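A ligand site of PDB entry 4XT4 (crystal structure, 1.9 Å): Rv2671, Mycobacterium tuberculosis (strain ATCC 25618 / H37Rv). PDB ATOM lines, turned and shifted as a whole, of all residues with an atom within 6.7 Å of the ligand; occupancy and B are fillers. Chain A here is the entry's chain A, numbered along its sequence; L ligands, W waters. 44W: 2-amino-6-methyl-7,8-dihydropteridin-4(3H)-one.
O of Asn 44 lies within hydrogen-bond range of N05 of the ligand (2.6 Å).
N03 of the ligand lies close to N of Phe 45 (3.5 Å).
A nitrogen (N01) of the ligand sits at hydrogen-bond distance from the side-chain carboxylate (OD1) of Asp 67, 2.5 Å away.
The backbone carbonyl oxygen (O) of Phe 45 lies within hydrogen-bond range of a nitrogen (N01) of the ligand, at 3.5 Å.
The side-chain amide oxygen of Asn 44 is in hydrogen-bond range of a nitrogen (N01) of the ligand.
The side-chain hydroxyl (OG1) of Thr 214 is in hydrogen-bond range of a nitrogen (N01) of the ligand.
A nitrogen (N19) of the ligand sits close to the side-chain carboxylate (OE1) of Glu 91 (3.4 Å).
Residues that only touch the ligand: Glu 193 (3.2 Å), Ile 46 (3.5 Å), Phe 71 (3.8 Å) and Ser 59 (3.8 Å).
Hydrophobic or aromatic side chains that line the ligand: Phe 45, Ile 46 and Phe 71.
Nine residues have an atom within 4 Å of the ligand: Asn 44, Phe 45, Ile 46, Ser 59, Asp 67, Phe 71, Glu 91, Glu 193 and Thr 214.
The side-chain carboxylate (OE1) of Glu 193 is in hydrogen-bond range of the side-chain hydroxyl (OH) of Tyr 93 (2.5 Å).
N of Asn 44 lies within hydrogen-bond range of O of Thr 192, 3.1 Å away.
The backbone NH (N) of Phe 45 lies within hydrogen-bond range of the backbone carbonyl oxygen (O) of Cys 212 (3.1 Å).
The backbone carbonyl oxygen (O) of Phe 45 sits at hydrogen-bond distance from the backbone NH (N) of Thr 214 (2.9 Å).
The side-chain hydroxyl (OG1) of Thr 214 lies within hydrogen-bond range of the side-chain carboxylate (OD1) of Asp 67.
The backbone carbonyl oxygen (O) of Cys 212 sits close to the side-chain amide oxygen (OD1) of Asn 44, 3.4 Å away.
N of Asp 67 is in hydrogen-bond range of OH of Tyr 252, 3.4 Å away.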
ATOM      1  N   ASN A  44      10.277   4.669  18.073  1.00  0.00           N
ATOM      2  CA  ASN A  44       9.622   4.924  19.348  1.00  0.00           C
ATOM      3  C   ASN A  44       9.995   6.307  19.845  1.00  0.00           C
ATOM      4  O   ASN A  44      11.174   6.595  20.060  1.00  0.00           O
ATOM      5  CB  ASN A  44      10.001   3.882  20.409  1.00  0.00           C
ATOM      6  CG  ASN A  44       9.202   4.051  21.695  1.00  0.00           C
ATOM      7  OD1 ASN A  44       8.062   4.532  21.681  1.00  0.00           O
ATOM      8  ND2 ASN A  44       9.799   3.634  22.833  1.00  0.00           N
ATOM      9  N   PHE A  45       8.989   7.137  20.075  1.00  0.00           N
ATOM     10  CA  PHE A  45       9.222   8.510  20.527  1.00  0.00           C
ATOM     11  C   PHE A  45       8.205   8.916  21.564  1.00  0.00           C
ATOM     12  O   PHE A  45       7.191   8.225  21.748  1.00  0.00           O
ATOM     13  CB  PHE A  45       9.175   9.475  19.339  1.00  0.00           C
ATOM     14  CG  PHE A  45      10.424   9.466  18.538  1.00  0.00           C
ATOM     15  CD1 PHE A  45      10.624   8.478  17.566  1.00  0.00           C
ATOM     16  CD2 PHE A  45      11.447  10.365  18.809  1.00  0.00           C
ATOM     17  CE1 PHE A  45      11.817   8.427  16.848  1.00  0.00           C
ATOM     18  CE2 PHE A  45      12.631  10.328  18.106  1.00  0.00           C
ATOM     19  CZ  PHE A  45      12.824   9.355  17.116  1.00  0.00           C
ATOM     20  N   ILE A  46       8.494  10.017  22.252  1.00  0.00           N
ATOM     21  CA  ILE A  46       7.521  10.599  23.178  1.00  0.00           C
ATOM     22  C   ILE A  46       7.375  12.078  22.851  1.00  0.00           C
ATOM     23  O   ILE A  46       8.359  12.734  22.473  1.00  0.00           O
ATOM     24  CB  ILE A  46       7.987  10.403  24.638  1.00  0.00           C
ATOM     25  CG1 ILE A  46       7.010  11.044  25.625  1.00  0.00           C
ATOM     26  CG2 ILE A  46       9.381  10.970  24.834  1.00  0.00           C
ATOM     27  CD1 ILE A  46       7.154  10.483  27.062  1.00  0.00           C
ATOM     28  N   THR A  58      16.299  16.907  26.756  1.00  0.00           N
ATOM     29  CA  THR A  58      15.986  15.485  26.850  1.00  0.00           C
ATOM     30  C   THR A  58      14.482  15.206  26.937  1.00  0.00           C
ATOM     31  O   THR A  58      13.685  16.119  27.159  1.00  0.00           O
ATOM     32  CB  THR A  58      16.683  14.856  28.078  1.00  0.00           C
ATOM     33  OG1 THR A  58      16.529  13.435  28.025  1.00  0.00           O
ATOM     34  CG2 THR A  58      16.094  15.389  29.361  1.00  0.00           C
ATOM     35  N   SER A  59      14.097  13.946  26.745  1.00  0.00           N
ATOM     36  CA  SER A  59      12.694  13.517  26.750  1.00  0.00           C
ATOM     37  C   SER A  59      12.195  13.099  28.139  1.00  0.00           C
ATOM     38  O   SER A  59      10.983  13.147  28.408  1.00  0.00           O
ATOM     39  CB  SER A  59      12.520  12.315  25.816  1.00  0.00           C
ATOM     40  OG  SER A  59      12.839  12.627  24.479  1.00  0.00           O
ATOM     41  N   GLY A  60      13.137  12.693  29.001  1.00  0.00           N
ATOM     42  CA  GLY A  60      12.847  11.964  30.221  1.00  0.00           C
ATOM     43  C   GLY A  60      11.863  12.581  31.208  1.00  0.00           C
ATOM     44  O   GLY A  60      11.139  11.850  31.895  1.00  0.00           O
ATOM     45  N   ALA A  63       8.484  11.321  30.672  1.00  0.00           N
ATOM     46  CA  ALA A  63       8.302   9.868  30.687  1.00  0.00           C
ATOM     47  C   ALA A  63       8.062   9.359  32.096  1.00  0.00           C
ATOM     48  O   ALA A  63       8.937   9.492  32.951  1.00  0.00           O
ATOM     49  CB  ALA A  63       9.535   9.180  30.106  1.00  0.00           C
ATOM     50  N   ASP A  67       5.652   4.752  30.385  1.00  0.00           N
ATOM     51  CA  ASP A  67       6.456   4.909  29.182  1.00  0.00           C
ATOM     52  C   ASP A  67       7.761   4.177  29.316  1.00  0.00           C
ATOM     53  O   ASP A  67       8.274   3.619  28.360  1.00  0.00           O
ATOM     54  CB  ASP A  67       6.707   6.389  28.861  1.00  0.00           C
ATOM     55  CG  ASP A  67       7.540   6.565  27.595  1.00  0.00           C
ATOM     56  OD1 ASP A  67       7.056   6.198  26.488  1.00  0.00           O
ATOM     57  OD2 ASP A  67       8.691   7.068  27.689  1.00  0.00           O
ATOM     58  N   ARG A  68       8.310   4.163  30.521  1.00  0.00           N
ATOM     59  CA  ARG A  68       9.557   3.415  30.727  1.00  0.00           C
ATOM     60  C   ARG A  68       9.340   1.938  30.454  1.00  0.00           C
ATOM     61  O   ARG A  68      10.205   1.251  29.868  1.00  0.00           O
ATOM     62  CB  ARG A  68      10.029   3.589  32.162  1.00  0.00           C
ATOM     63  CG  ARG A  68      10.555   4.962  32.472  1.00  0.00           C
ATOM     64  CD  ARG A  68      11.018   5.003  33.924  1.00  0.00           C
ATOM     65  NE  ARG A  68      11.764   6.212  34.197  1.00  0.00           N
ATOM     66  CZ  ARG A  68      12.984   6.235  34.732  1.00  0.00           C
ATOM     67  NH1 ARG A  68      13.594   5.106  35.073  1.00  0.00           N
ATOM     68  NH2 ARG A  68      13.571   7.401  34.941  1.00  0.00           N
ATOM     69  N   VAL A  70       6.974   0.577  28.424  1.00  0.00           N
ATOM     70  CA  VAL A  70       6.857   0.381  26.980  1.00  0.00           C
ATOM     71  C   VAL A  70       8.219   0.502  26.268  1.00  0.00           C
ATOM     72  O   VAL A  70       8.571  -0.290  25.389  1.00  0.00           O
ATOM     73  CB  VAL A  70       5.778   1.343  26.377  1.00  0.00           C
ATOM     74  CG1 VAL A  70       5.696   1.199  24.856  1.00  0.00           C
ATOM     75  CG2 VAL A  70       4.435   1.018  26.964  1.00  0.00           C
ATOM     76  N   PHE A  71       9.008   1.491  26.686  1.00  0.00           N
ATOM     77  CA  PHE A  71      10.311   1.759  26.080  1.00  0.00           C
ATOM     78  C   PHE A  71      11.242   0.532  26.215  1.00  0.00           C
ATOM     79  O   PHE A  71      11.878   0.074  25.230  1.00  0.00           O
ATOM     80  CB  PHE A  71      10.891   3.001  26.782  1.00  0.00           C
ATOM     81  CG  PHE A  71      12.235   3.421  26.284  1.00  0.00           C
ATOM     82  CD1 PHE A  71      13.399   2.923  26.856  1.00  0.00           C
ATOM     83  CD2 PHE A  71      12.341   4.357  25.259  1.00  0.00           C
ATOM     84  CE1 PHE A  71      14.651   3.332  26.393  1.00  0.00           C
ATOM     85  CE2 PHE A  71      13.579   4.766  24.795  1.00  0.00           C
ATOM     86  CZ  PHE A  71      14.744   4.254  25.373  1.00  0.00           C
ATOM     87  N   LEU A  74       9.950  -2.401  23.944  1.00  0.00           N
ATOM     88  CA  LEU A  74      10.307  -2.275  22.538  1.00  0.00           C
ATOM     89  C   LEU A  74      11.790  -2.582  22.344  1.00  0.00           C
ATOM     90  O   LEU A  74      12.158  -3.203  21.345  1.00  0.00           O
ATOM     91  CB  LEU A  74       9.965  -0.881  21.989  1.00  0.00           C
ATOM     92  CG  LEU A  74       8.469  -0.582  22.132  1.00  0.00           C
ATOM     93  CD1 LEU A  74       8.061   0.746  21.478  1.00  0.00           C
ATOM     94  CD2 LEU A  74       7.662  -1.727  21.542  1.00  0.00           C
ATOM     95  N   THR A  87      21.973  12.099  19.175  1.00  0.00           N
ATOM     96  CA  THR A  87      21.177  11.642  20.317  1.00  0.00           C
ATOM     97  C   THR A  87      22.053  10.784  21.248  1.00  0.00           C
ATOM     98  O   THR A  87      21.883  10.825  22.476  1.00  0.00           O
ATOM     99  CB  THR A  87      19.889  10.906  19.861  1.00  0.00           C
ATOM    100  OG1 THR A  87      18.947  10.879  20.933  1.00  0.00           O
ATOM    101  CG2 THR A  87      20.182   9.484  19.431  1.00  0.00           C
ATOM    102  N   GLU A  91      21.658  12.228  24.786  1.00  0.00           N
ATOM    103  CA  GLU A  91      20.969  11.472  25.826  1.00  0.00           C
ATOM    104  C   GLU A  91      21.907  10.564  26.608  1.00  0.00           C
ATOM    105  O   GLU A  91      21.479   9.892  27.555  1.00  0.00           O
ATOM    106  CB  GLU A  91      19.756  10.689  25.296  1.00  0.00           C
ATOM    107  CG  GLU A  91      18.668  10.589  26.406  1.00  0.00           C
ATOM    108  CD  GLU A  91      17.601   9.548  26.186  1.00  0.00           C
ATOM    109  OE1 GLU A  91      16.486   9.959  25.810  1.00  0.00           O
ATOM    110  OE2 GLU A  91      17.844   8.312  26.406  1.00  0.00           O
ATOM    111  N   TYR A  93      23.779   7.831  25.652  1.00  0.00           N
ATOM    112  CA  TYR A  93      23.629   6.404  25.416  1.00  0.00           C
ATOM    113  C   TYR A  93      24.857   5.660  25.904  1.00  0.00           C
ATOM    114  O   TYR A  93      25.989   5.991  25.536  1.00  0.00           O
ATOM    115  CB  TYR A  93      23.420   6.106  23.926  1.00  0.00           C
ATOM    116  CG  TYR A  93      21.982   6.161  23.478  1.00  0.00           C
ATOM    117  CD1 TYR A  93      21.232   7.316  23.648  1.00  0.00           C
ATOM    118  CD2 TYR A  93      21.379   5.057  22.878  1.00  0.00           C
ATOM    119  CE1 TYR A  93      19.914   7.383  23.233  1.00  0.00           C
ATOM    120  CE2 TYR A  93      20.062   5.120  22.454  1.00  0.00           C
ATOM    121  CZ  TYR A  93      19.333   6.273  22.636  1.00  0.00           C
ATOM    122  OH  TYR A  93      18.014   6.357  22.224  1.00  0.00           O
ATOM    123  N   THR A 192      14.228   2.317  16.031  1.00  0.00           N
ATOM    124  CA  THR A 192      15.035   3.522  16.122  1.00  0.00           C
ATOM    125  C   THR A 192      14.525   4.448  17.186  1.00  0.00           C
ATOM    126  O   THR A 192      13.311   4.586  17.380  1.00  0.00           O
ATOM    127  CB  THR A 192      15.120   4.306  14.780  1.00  0.00           C
ATOM    128  OG1 THR A 192      15.978   5.437  14.961  1.00  0.00           O
ATOM    129  CG2 THR A 192      13.741   4.792  14.336  1.00  0.00           C
ATOM    130  N   GLU A 193      15.443   5.121  17.874  1.00  0.00           N
ATOM    131  CA  GLU A 193      14.996   6.039  18.934  1.00  0.00           C
ATOM    132  C   GLU A 193      15.391   7.474  18.639  1.00  0.00           C
ATOM    133  O   GLU A 193      15.333   8.335  19.509  1.00  0.00           O
ATOM    134  CB  GLU A 193      15.503   5.611  20.325  1.00  0.00           C
ATOM    135  CG  GLU A 193      14.850   4.326  20.849  1.00  0.00           C
ATOM    136  CD  GLU A 193      15.605   3.697  22.002  1.00  0.00           C
ATOM    137  OE1 GLU A 193      16.716   4.168  22.318  1.00  0.00           O
ATOM    138  OE2 GLU A 193      15.085   2.714  22.581  1.00  0.00           O
ATOM    139  N   GLY A 194      15.766   7.749  17.386  1.00  0.00           N
ATOM    140  CA  GLY A 194      16.087   9.115  16.999  1.00  0.00           C
ATOM    141  C   GLY A 194      17.577   9.316  16.760  1.00  0.00           C
ATOM    142  O   GLY A 194      18.299   8.343  16.496  1.00  0.00           O
ATOM    143  N   GLY A 195      18.049  10.564  16.851  1.00  0.00           N
ATOM    144  CA  GLY A 195      17.225  11.700  17.224  1.00  0.00           C
ATOM    145  C   GLY A 195      16.388  12.261  16.098  1.00  0.00           C
ATOM    146  O   GLY A 195      16.100  11.569  15.115  1.00  0.00           O
ATOM    147  N   CYS A 212       5.671   4.141  17.022  1.00  0.00           N
ATOM    148  CA  CYS A 212       5.040   4.032  18.331  1.00  0.00           C
ATOM    149  C   CYS A 212       5.262   5.369  18.997  1.00  0.00           C
ATOM    150  O   CYS A 212       6.386   5.842  19.093  1.00  0.00           O
ATOM    151  CB  CYS A 212       5.661   2.916  19.161  1.00  0.00           C
ATOM    152  SG  CYS A 212       5.405   1.273  18.391  1.00  0.00           S
ATOM    153  N   LEU A 213       4.184   6.004  19.433  1.00  0.00           N
ATOM    154  CA  LEU A 213       4.360   7.322  19.973  1.00  0.00           C
ATOM    155  C   LEU A 213       3.648   7.418  21.296  1.00  0.00           C
ATOM    156  O   LEU A 213       2.449   7.125  21.379  1.00  0.00           O
ATOM    157  CB  LEU A 213       3.767   8.366  19.002  1.00  0.00           C
ATOM    158  CG  LEU A 213       3.768   9.783  19.567  1.00  0.00           C
ATOM    159  CD1 LEU A 213       5.193  10.348  19.622  1.00  0.00           C
ATOM    160  CD2 LEU A 213       2.875  10.664  18.722  1.00  0.00           C
ATOM    161  N   THR A 214       4.380   7.824  22.318  1.00  0.00           N
ATOM    162  CA  THR A 214       3.808   8.125  23.620  1.00  0.00           C
ATOM    163  C   THR A 214       3.430   9.598  23.605  1.00  0.00           C
ATOM    164  O   THR A 214       4.272  10.476  23.384  1.00  0.00           O
ATOM    165  CB  THR A 214       4.796   7.834  24.728  1.00  0.00           C
ATOM    166  OG1 THR A 214       5.028   6.426  24.794  1.00  0.00           O
ATOM    167  CG2 THR A 214       4.243   8.310  26.071  1.00  0.00           C
ATOM    168  N   ARG A 225      11.687  21.525  20.277  1.00  0.00           N
ATOM    169  CA  ARG A 225      11.633  21.030  18.906  1.00  0.00           C
ATOM    170  C   ARG A 225      10.631  19.894  18.831  1.00  0.00           C
ATOM    171  O   ARG A 225      10.223  19.350  19.852  1.00  0.00           O
ATOM    172  CB  ARG A 225      13.010  20.504  18.499  1.00  0.00           C
ATOM    173  CG  ARG A 225      13.484  19.345  19.364  1.00  0.00           C
ATOM    174  CD  ARG A 225      14.724  18.643  18.800  1.00  0.00           C
ATOM    175  NE  ARG A 225      15.266  17.650  19.736  1.00  0.00           N
ATOM    176  CZ  ARG A 225      14.766  16.426  19.920  1.00  0.00           C
ATOM    177  NH1 ARG A 225      13.686  16.041  19.247  1.00  0.00           N
ATOM    178  NH2 ARG A 225      15.345  15.585  20.777  1.00  0.00           N
ATOM    179  N   TYR A 252      -0.424   5.555  24.677  1.00  0.00           N
ATOM    180  CA  TYR A 252       0.651   4.799  24.043  1.00  0.00           C
ATOM    181  C   TYR A 252       0.127   4.312  22.726  1.00  0.00           C
ATOM    182  O   TYR A 252      -0.678   3.362  22.684  1.00  0.00           O
ATOM    183  CB  TYR A 252       1.110   3.622  24.938  1.00  0.00           C
ATOM    184  CG  TYR A 252       1.468   4.137  26.313  1.00  0.00           C
ATOM    185  CD1 TYR A 252       2.728   4.670  26.563  1.00  0.00           C
ATOM    186  CD2 TYR A 252       0.533   4.156  27.331  1.00  0.00           C
ATOM    187  CE1 TYR A 252       3.046   5.189  27.813  1.00  0.00           C
ATOM    188  CE2 TYR A 252       0.851   4.662  28.587  1.00  0.00           C
ATOM    189  CZ  TYR A 252       2.098   5.182  28.810  1.00  0.00           C
ATOM    190  OH  TYR A 252       2.409   5.690  30.054  1.00  0.00           O
HETATM  191  N01 44W L   1       8.466   6.487  24.470  1.00  0.00           N
HETATM  192  C02 44W L   1       9.736   7.077  24.420  1.00  0.00           C
HETATM  193  N03 44W L   1      10.410   7.123  23.240  1.00  0.00           N
HETATM  194  C04 44W L   1      11.678   7.721  23.274  1.00  0.00           C
HETATM  195  N05 44W L   1      12.417   7.764  22.065  1.00  0.00           N
HETATM  196  C06 44W L   1      13.364   8.929  21.971  1.00  0.00           C
HETATM  197  C07 44W L   1      14.132   9.199  23.254  1.00  0.00           C
HETATM  198  C08 44W L   1      15.556   9.835  23.157  1.00  0.00           C
HETATM  199  N19 44W L   1      13.576   8.896  24.424  1.00  0.00           N
HETATM  200  C20 44W L   1      12.301   8.288  24.384  1.00  0.00           C
HETATM  201  C21 44W L   1      11.575   8.249  25.668  1.00  0.00           C
HETATM  202  O22 44W L   1      11.888   8.655  26.739  1.00  0.00           O
HETATM  203  N23 44W L   1      10.282   7.617  25.561  1.00  0.00           N
HETATM  204  O   HOH W   1       7.565   3.790  25.021  1.00  0.00           O
